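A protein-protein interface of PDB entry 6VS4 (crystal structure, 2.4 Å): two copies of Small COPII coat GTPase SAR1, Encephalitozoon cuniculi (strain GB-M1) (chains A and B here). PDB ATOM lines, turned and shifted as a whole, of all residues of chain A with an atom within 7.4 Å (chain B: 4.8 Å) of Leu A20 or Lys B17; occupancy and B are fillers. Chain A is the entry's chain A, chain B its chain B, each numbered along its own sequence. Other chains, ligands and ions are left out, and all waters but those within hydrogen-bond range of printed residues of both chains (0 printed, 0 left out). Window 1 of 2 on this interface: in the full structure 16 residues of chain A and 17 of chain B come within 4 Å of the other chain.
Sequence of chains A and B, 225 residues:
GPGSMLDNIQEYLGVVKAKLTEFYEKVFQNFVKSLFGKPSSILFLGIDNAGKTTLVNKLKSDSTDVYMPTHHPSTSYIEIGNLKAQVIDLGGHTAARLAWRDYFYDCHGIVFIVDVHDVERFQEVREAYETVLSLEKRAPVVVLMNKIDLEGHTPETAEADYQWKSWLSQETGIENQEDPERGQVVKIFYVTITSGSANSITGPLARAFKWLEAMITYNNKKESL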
ATOM      1  N   LEU A  13       3.240  -8.646  13.375  1.00  0.00           N
ATOM      2  CA  LEU A  13       3.531 -10.025  13.750  1.00  0.00           C
ATOM      3  C   LEU A  13       4.671 -10.082  14.763  1.00  0.00           C
ATOM      4  O   LEU A  13       4.622 -10.857  15.726  1.00  0.00           O
ATOM      5  CB  LEU A  13       3.867 -10.844  12.504  1.00  0.00           C
ATOM      6  CG  LEU A  13       2.743 -11.107  11.510  1.00  0.00           C
ATOM      7  CD1 LEU A  13       3.299 -11.707  10.223  1.00  0.00           C
ATOM      8  CD2 LEU A  13       1.770 -12.070  12.145  1.00  0.00           C
ATOM      9  N   GLY A  14       5.685  -9.233  14.591  1.00  0.00           N
ATOM     10  CA  GLY A  14       6.791  -9.225  15.533  1.00  0.00           C
ATOM     11  C   GLY A  14       6.402  -8.704  16.902  1.00  0.00           C
ATOM     12  O   GLY A  14       6.810  -9.265  17.926  1.00  0.00           O
ATOM     13  N   VAL A  15       5.607  -7.632  16.944  1.00  0.00           N
ATOM     14  CA  VAL A  15       5.155  -7.077  18.220  1.00  0.00           C
ATOM     15  C   VAL A  15       4.326  -8.103  18.985  1.00  0.00           C
ATOM     16  O   VAL A  15       4.511  -8.304  20.194  1.00  0.00           O
ATOM     17  CB  VAL A  15       4.379  -5.768  17.976  1.00  0.00           C
ATOM     18  CG1 VAL A  15       3.423  -5.452  19.135  1.00  0.00           C
ATOM     19  CG2 VAL A  15       5.357  -4.618  17.746  1.00  0.00           C
ATOM     20  N   VAL A  16       3.420  -8.789  18.292  1.00  0.00           N
ATOM     21  CA  VAL A  16       2.589  -9.782  18.961  1.00  0.00           C
ATOM     22  C   VAL A  16       3.440 -10.941  19.450  1.00  0.00           C
ATOM     23  O   VAL A  16       3.287 -11.403  20.586  1.00  0.00           O
ATOM     24  CB  VAL A  16       1.465 -10.263  18.034  1.00  0.00           C
ATOM     25  CG1 VAL A  16       0.692 -11.395  18.708  1.00  0.00           C
ATOM     26  CG2 VAL A  16       0.564  -9.098  17.671  1.00  0.00           C
ATOM     27  N   LYS A  17       4.353 -11.425  18.604  1.00  0.00           N
ATOM     28  CA  LYS A  17       5.232 -12.510  19.020  1.00  0.00           C
ATOM     29  C   LYS A  17       6.022 -12.118  20.257  1.00  0.00           C
ATOM     30  O   LYS A  17       6.168 -12.918  21.187  1.00  0.00           O
ATOM     31  CB  LYS A  17       6.178 -12.894  17.886  1.00  0.00           C
ATOM     32  CG  LYS A  17       5.540 -13.742  16.812  1.00  0.00           C
ATOM     33  CD  LYS A  17       6.465 -13.895  15.617  1.00  0.00           C
ATOM     34  CE  LYS A  17       7.770 -14.575  16.014  1.00  0.00           C
ATOM     35  NZ  LYS A  17       8.530 -15.002  14.807  1.00  0.00           N
ATOM     36  N   ALA A  18       6.477 -10.867  20.321  1.00  0.00           N
ATOM     37  CA  ALA A  18       7.220 -10.427  21.495  1.00  0.00           C
ATOM     38  C   ALA A  18       6.344 -10.445  22.744  1.00  0.00           C
ATOM     39  O   ALA A  18       6.799 -10.859  23.818  1.00  0.00           O
ATOM     40  CB  ALA A  18       7.795  -9.033  21.259  1.00  0.00           C
ATOM     41  N   LYS A  19       5.080 -10.015  22.629  1.00  0.00           N
ATOM     42  CA  LYS A  19       4.198 -10.071  23.794  1.00  0.00           C
ATOM     43  C   LYS A  19       3.937 -11.513  24.202  1.00  0.00           C
ATOM     44  O   LYS A  19       3.904 -11.823  25.397  1.00  0.00           O
ATOM     45  CB  LYS A  19       2.873  -9.351  23.525  1.00  0.00           C
ATOM     46  CG  LYS A  19       2.994  -7.870  23.207  1.00  0.00           C
ATOM     47  CD  LYS A  19       3.500  -7.050  24.391  1.00  0.00           C
ATOM     48  CE  LYS A  19       3.559  -5.562  24.021  1.00  0.00           C
ATOM     49  NZ  LYS A  19       4.125  -4.718  25.120  1.00  0.00           N
ATOM     50  N   LEU A  20       3.797 -12.416  23.224  1.00  0.00           N
ATOM     51  CA  LEU A  20       3.600 -13.827  23.546  1.00  0.00           C
ATOM     52  C   LEU A  20       4.806 -14.404  24.282  1.00  0.00           C
ATOM     53  O   LEU A  20       4.652 -15.196  25.221  1.00  0.00           O
ATOM     54  CB  LEU A  20       3.330 -14.625  22.274  1.00  0.00           C
ATOM     55  CG  LEU A  20       2.085 -14.287  21.453  1.00  0.00           C
ATOM     56  CD1 LEU A  20       1.935 -15.253  20.288  1.00  0.00           C
ATOM     57  CD2 LEU A  20       0.840 -14.302  22.328  1.00  0.00           C
ATOM     58  N   THR A  21       6.013 -13.994  23.891  1.00  0.00           N
ATOM     59  CA  THR A  21       7.216 -14.480  24.561  1.00  0.00           C
ATOM     60  C   THR A  21       7.290 -13.986  26.009  1.00  0.00           C
ATOM     61  O   THR A  21       7.574 -14.767  26.924  1.00  0.00           O
ATOM     62  CB  THR A  21       8.441 -14.061  23.757  1.00  0.00           C
ATOM     63  OG1 THR A  21       8.382 -14.688  22.474  1.00  0.00           O
ATOM     64  CG2 THR A  21       9.733 -14.505  24.458  1.00  0.00           C
ATOM     65  N   GLU A  22       7.014 -12.695  26.242  1.00  0.00           N
ATOM     66  CA  GLU A  22       6.973 -12.178  27.610  1.00  0.00           C
ATOM     67  C   GLU A  22       5.939 -12.919  28.445  1.00  0.00           C
ATOM     68  O   GLU A  22       6.189 -13.252  29.609  1.00  0.00           O
ATOM     69  CB  GLU A  22       6.627 -10.689  27.629  1.00  0.00           C
ATOM     70  CG  GLU A  22       7.563  -9.731  26.954  1.00  0.00           C
ATOM     71  CD  GLU A  22       7.037  -8.303  27.055  1.00  0.00           C
ATOM     72  OE1 GLU A  22       6.993  -7.599  26.021  1.00  0.00           O
ATOM     73  OE2 GLU A  22       6.638  -7.897  28.172  1.00  0.00           O
ATOM     74  N   PHE A  23       4.762 -13.164  27.862  1.00  0.00           N
ATOM     75  CA  PHE A  23       3.698 -13.885  28.546  1.00  0.00           C
ATOM     76  C   PHE A  23       4.142 -15.302  28.897  1.00  0.00           C
ATOM     77  O   PHE A  23       3.975 -15.757  30.035  1.00  0.00           O
ATOM     78  CB  PHE A  23       2.470 -13.900  27.627  1.00  0.00           C
ATOM     79  CG  PHE A  23       1.190 -14.311  28.288  1.00  0.00           C
ATOM     80  CD1 PHE A  23       1.157 -14.724  29.610  1.00  0.00           C
ATOM     81  CD2 PHE A  23       0.004 -14.283  27.569  1.00  0.00           C
ATOM     82  CE1 PHE A  23      -0.038 -15.097  30.202  1.00  0.00           C
ATOM     83  CE2 PHE A  23      -1.191 -14.651  28.152  1.00  0.00           C
ATOM     84  CZ  PHE A  23      -1.211 -15.061  29.473  1.00  0.00           C
ATOM     85  N   TYR A  24       4.766 -15.985  27.938  1.00  0.00           N
ATOM     86  CA  TYR A  24       5.276 -17.330  28.161  1.00  0.00           C
ATOM     87  C   TYR A  24       6.250 -17.354  29.329  1.00  0.00           C
ATOM     88  O   TYR A  24       6.174 -18.233  30.196  1.00  0.00           O
ATOM     89  CB  TYR A  24       5.948 -17.813  26.873  1.00  0.00           C
ATOM     90  CG  TYR A  24       6.214 -19.297  26.760  1.00  0.00           C
ATOM     91  CD1 TYR A  24       5.316 -20.134  26.111  1.00  0.00           C
ATOM     92  CD2 TYR A  24       7.399 -19.852  27.248  1.00  0.00           C
ATOM     93  CE1 TYR A  24       5.564 -21.489  25.987  1.00  0.00           C
ATOM     94  CE2 TYR A  24       7.657 -21.202  27.133  1.00  0.00           C
ATOM     95  CZ  TYR A  24       6.740 -22.015  26.501  1.00  0.00           C
ATOM     96  OH  TYR A  24       7.007 -23.357  26.390  1.00  0.00           O
ATOM     97  N   GLU A  25       7.129 -16.354  29.406  1.00  0.00           N
ATOM     98  CA  GLU A  25       8.089 -16.297  30.504  1.00  0.00           C
ATOM     99  C   GLU A  25       7.401 -15.996  31.826  1.00  0.00           C
ATOM    100  O   GLU A  25       7.808 -16.512  32.873  1.00  0.00           O
ATOM    101  CB  GLU A  25       9.170 -15.261  30.209  1.00  0.00           C
ATOM    102  CG  GLU A  25      10.130 -15.678  29.108  1.00  0.00           C
ATOM    103  CD  GLU A  25      10.921 -14.511  28.541  1.00  0.00           C
ATOM    104  OE1 GLU A  25      10.782 -13.385  29.072  1.00  0.00           O
ATOM    105  OE2 GLU A  25      11.701 -14.729  27.582  1.00  0.00           O
ATOM    106  N   LYS A  26       6.375 -15.139  31.800  1.00  0.00           N
ATOM    107  CA  LYS A  26       5.676 -14.777  33.030  1.00  0.00           C
ATOM    108  C   LYS A  26       5.029 -15.994  33.676  1.00  0.00           C
ATOM    109  O   LYS A  26       5.077 -16.151  34.900  1.00  0.00           O
ATOM    110  CB  LYS A  26       4.619 -13.711  32.734  1.00  0.00           C
ATOM    111  CG  LYS A  26       3.878 -13.209  33.971  1.00  0.00           C
ATOM    112  CD  LYS A  26       4.794 -12.382  34.857  1.00  0.00           C
ATOM    113  CE  LYS A  26       4.043 -11.724  36.003  1.00  0.00           C
ATOM    114  NZ  LYS A  26       3.761 -12.658  37.121  1.00  0.00           N
ATOM    115  N   GLY A 196      14.341 -20.592  24.982  1.00  0.00           N
ATOM    116  CA  GLY A 196      13.012 -20.111  25.315  1.00  0.00           C
ATOM    117  C   GLY A 196      12.097 -21.209  25.812  1.00  0.00           C
ATOM    118  O   GLY A 196      11.231 -20.962  26.662  1.00  0.00           O
ATOM    119  N   LEU B  13       0.175 -20.454  23.593  1.00  0.00           N
ATOM    120  CA  LEU B  13       1.025 -19.336  23.183  1.00  0.00           C
ATOM    121  C   LEU B  13       2.100 -19.788  22.207  1.00  0.00           C
ATOM    122  O   LEU B  13       2.456 -19.056  21.281  1.00  0.00           O
ATOM    123  CB  LEU B  13       1.680 -18.677  24.392  1.00  0.00           C
ATOM    124  CG  LEU B  13       0.744 -17.987  25.376  1.00  0.00           C
ATOM    125  CD1 LEU B  13       1.543 -17.485  26.583  1.00  0.00           C
ATOM    126  CD2 LEU B  13      -0.032 -16.882  24.702  1.00  0.00           C
ATOM    127  N   GLY B  14       2.645 -20.987  22.415  1.00  0.00           N
ATOM    128  CA  GLY B  14       3.655 -21.497  21.504  1.00  0.00           C
ATOM    129  C   GLY B  14       3.085 -21.860  20.149  1.00  0.00           C
ATOM    130  O   GLY B  14       3.715 -21.617  19.118  1.00  0.00           O
ATOM    131  N   VAL B  15       1.899 -22.467  20.132  1.00  0.00           N
ATOM    132  CA  VAL B  15       1.253 -22.796  18.866  1.00  0.00           C
ATOM    133  C   VAL B  15       0.991 -21.527  18.061  1.00  0.00           C
ATOM    134  O   VAL B  15       1.246 -21.472  16.850  1.00  0.00           O
ATOM    135  CB  VAL B  15      -0.040 -23.586  19.130  1.00  0.00           C
ATOM    136  CG1 VAL B  15      -0.990 -23.457  17.957  1.00  0.00           C
ATOM    137  CG2 VAL B  15       0.289 -25.041  19.411  1.00  0.00           C
ATOM    138  N   VAL B  16       0.507 -20.479  18.728  1.00  0.00           N
ATOM    139  CA  VAL B  16       0.231 -19.218  18.048  1.00  0.00           C
ATOM    140  C   VAL B  16       1.517 -18.582  17.536  1.00  0.00           C
ATOM    141  O   VAL B  16       1.576 -18.095  16.403  1.00  0.00           O
ATOM    142  CB  VAL B  16      -0.509 -18.261  18.994  1.00  0.00           C
ATOM    143  CG1 VAL B  16      -0.654 -16.878  18.350  1.00  0.00           C
ATOM    144  CG2 VAL B  16      -1.853 -18.848  19.389  1.00  0.00           C
ATOM    145  N   LYS B  17       2.556 -18.556  18.369  1.00  0.00           N
ATOM    146  CA  LYS B  17       3.812 -17.942  17.955  1.00  0.00           C
ATOM    147  C   LYS B  17       4.376 -18.617  16.707  1.00  0.00           C
ATOM    148  O   LYS B  17       4.882 -17.941  15.805  1.00  0.00           O
ATOM    149  CB  LYS B  17       4.810 -17.978  19.111  1.00  0.00           C
ATOM    150  CG  LYS B  17       6.051 -17.149  18.883  1.00  0.00           C
ATOM    151  CD  LYS B  17       6.800 -16.909  20.187  1.00  0.00           C
ATOM    152  CE  LYS B  17       8.304 -16.981  19.988  1.00  0.00           C
ATOM    153  NZ  LYS B  17       8.782 -18.390  20.042  1.00  0.00           N
ATOM    154  N   ALA B  18       4.262 -19.944  16.620  1.00  0.00           N
ATOM    155  CA  ALA B  18       4.724 -20.653  15.428  1.00  0.00           C
ATOM    156  C   ALA B  18       3.879 -20.309  14.206  1.00  0.00           C
ATOM    157  O   ALA B  18       4.412 -20.168  13.101  1.00  0.00           O
ATOM    158  CB  ALA B  18       4.725 -22.167  15.669  1.00  0.00           C
ATOM    159  N   LYS B  19       2.558 -20.195  14.373  1.00  0.00           N
ATOM    160  CA  LYS B  19       1.711 -19.818  13.243  1.00  0.00           C
ATOM    161  C   LYS B  19       1.990 -18.387  12.796  1.00  0.00           C
ATOM    162  O   LYS B  19       1.963 -18.092  11.597  1.00  0.00           O
ATOM    163  CB  LYS B  19       0.235 -19.998  13.607  1.00  0.00           C
ATOM    164  CG  LYS B  19      -0.740 -19.818  12.445  1.00  0.00           C
ATOM    165  CD  LYS B  19      -0.423 -20.769  11.310  1.00  0.00           C
ATOM    166  CE  LYS B  19      -1.464 -20.721  10.199  1.00  0.00           C
ATOM    167  NZ  LYS B  19      -2.592 -21.663  10.444  1.00  0.00           N
ATOM    168  N   LEU B  20       2.245 -17.478  13.739  1.00  0.00           N
ATOM    169  CA  LEU B  20       2.610 -16.115  13.359  1.00  0.00           C
ATOM    170  C   LEU B  20       3.947 -16.101  12.618  1.00  0.00           C
ATOM    171  O   LEU B  20       4.136 -15.332  11.666  1.00  0.00           O
ATOM    172  CB  LEU B  20       2.648 -15.205  14.591  1.00  0.00           C
ATOM    173  CG  LEU B  20       1.345 -14.967  15.388  1.00  0.00           C
ATOM    174  CD1 LEU B  20       1.555 -13.931  16.481  1.00  0.00           C
ATOM    175  CD2 LEU B  20       0.176 -14.554  14.506  1.00  0.00           C
ATOM    176  N   THR B  21       4.878 -16.968  13.023  1.00  0.00           N
ATOM    177  CA  THR B  21       6.153 -17.072  12.321  1.00  0.00           C
ATOM    178  C   THR B  21       5.938 -17.531  10.887  1.00  0.00           C
ATOM    179  O   THR B  21       6.535 -16.983   9.953  1.00  0.00           O
ATOM    180  CB  THR B  21       7.080 -18.036  13.058  1.00  0.00           C
ATOM    181  OG1 THR B  21       7.411 -17.487  14.336  1.00  0.00           O
ATOM    182  CG2 THR B  21       8.370 -18.277  12.262  1.00  0.00           C
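Leu A13 touches Leu B20. Leu B20 touches Val A16 (CD1 to CG1, 3.5 Å). CG of Lys A17 touches CB of Leu B20, at 3.9 Å. CD2 of Leu B13 touches CD2 of Leu A20 (3.6 Å). CD1 of Leu A20 touches CG1 of Val B16, 3.6 Å away. CD1 of Leu A20 touches N of Lys B17, at 3.9 Å. OG1 of Thr A21 touches CE of Lys B17, 3.4 Å away. Leu B13 touches Phe A23 (CD1 to CG, 3.6 Å). Tyr A24 touches Leu B13 (N to CD1, 3.8 Å).
Leu A20 touches just these residues of chain B: Leu B13, Val B16 and Lys B17. Of the printed residues of chain A, Lys B17 touches Leu A20 (3.9 Å) and Thr A21 (3.4 Å). Of the printed residues of chain B, Leu A13 touches Leu B20. Of the printed residues of chain B, Thr A21 touches Lys B17 (3.4 Å). Of the printed residues of chain A, Thr B21 touches Lys A17 (2.8 Å). Printed residues of chain B within 4 Å of Tyr A24: Leu B13 (3.8 Å). Glu A22 touches none of the printed residues of chain B. Ala B18 touches none of the printed residues of chain A. The nearest residue of chain B that does not touch Leu A20 is Leu B20 (4.05 Å).
The side-chain hydroxyl (OG1) of Thr B21 is in hydrogen-bond range of the side-chain amino group (NZ) of Lys A17 (2.8 Å).
Of the 9 printed residues of chain B, 5 touch a printed residue of chain A. Hydrophobic or aromatic side chains of chain B that line the printed part of chain A: Leu B13, Val B16 and Leu B20. Of the 15 printed residues of chain A, 7 touch a printed residue of chain B. Among the printed residues, 10 pairs touch across the chains. Among the printed residues, no Asp or Glu carboxylate lies within 4 Å of a Lys or Arg side-chain nitrogen of the other chain.
Leu A13 touches Leu B20, and with the chains exchanged Leu A20 touches Leu B13. Val A16 touches Leu B20, and with the chains exchanged Leu A20 touches Val B16. Lys A17 touches Leu B20, and with the chains exchanged Leu A20 touches Lys B17. Lys A17 touches Thr B21, and with the chains exchanged Thr A21 touches Lys B17. Positions printed for both chains: 13, 14, 15, 16, 17, 18, 19, 20 and 21.
O of Lys A17 is in hydrogen-bond range of OG1 of Thr A21. The backbone carbonyl oxygen (O) of Lys B17 is in hydrogen-bond range of the side-chain hydroxyl (OG1) of Thr B21 (3.0 Å).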
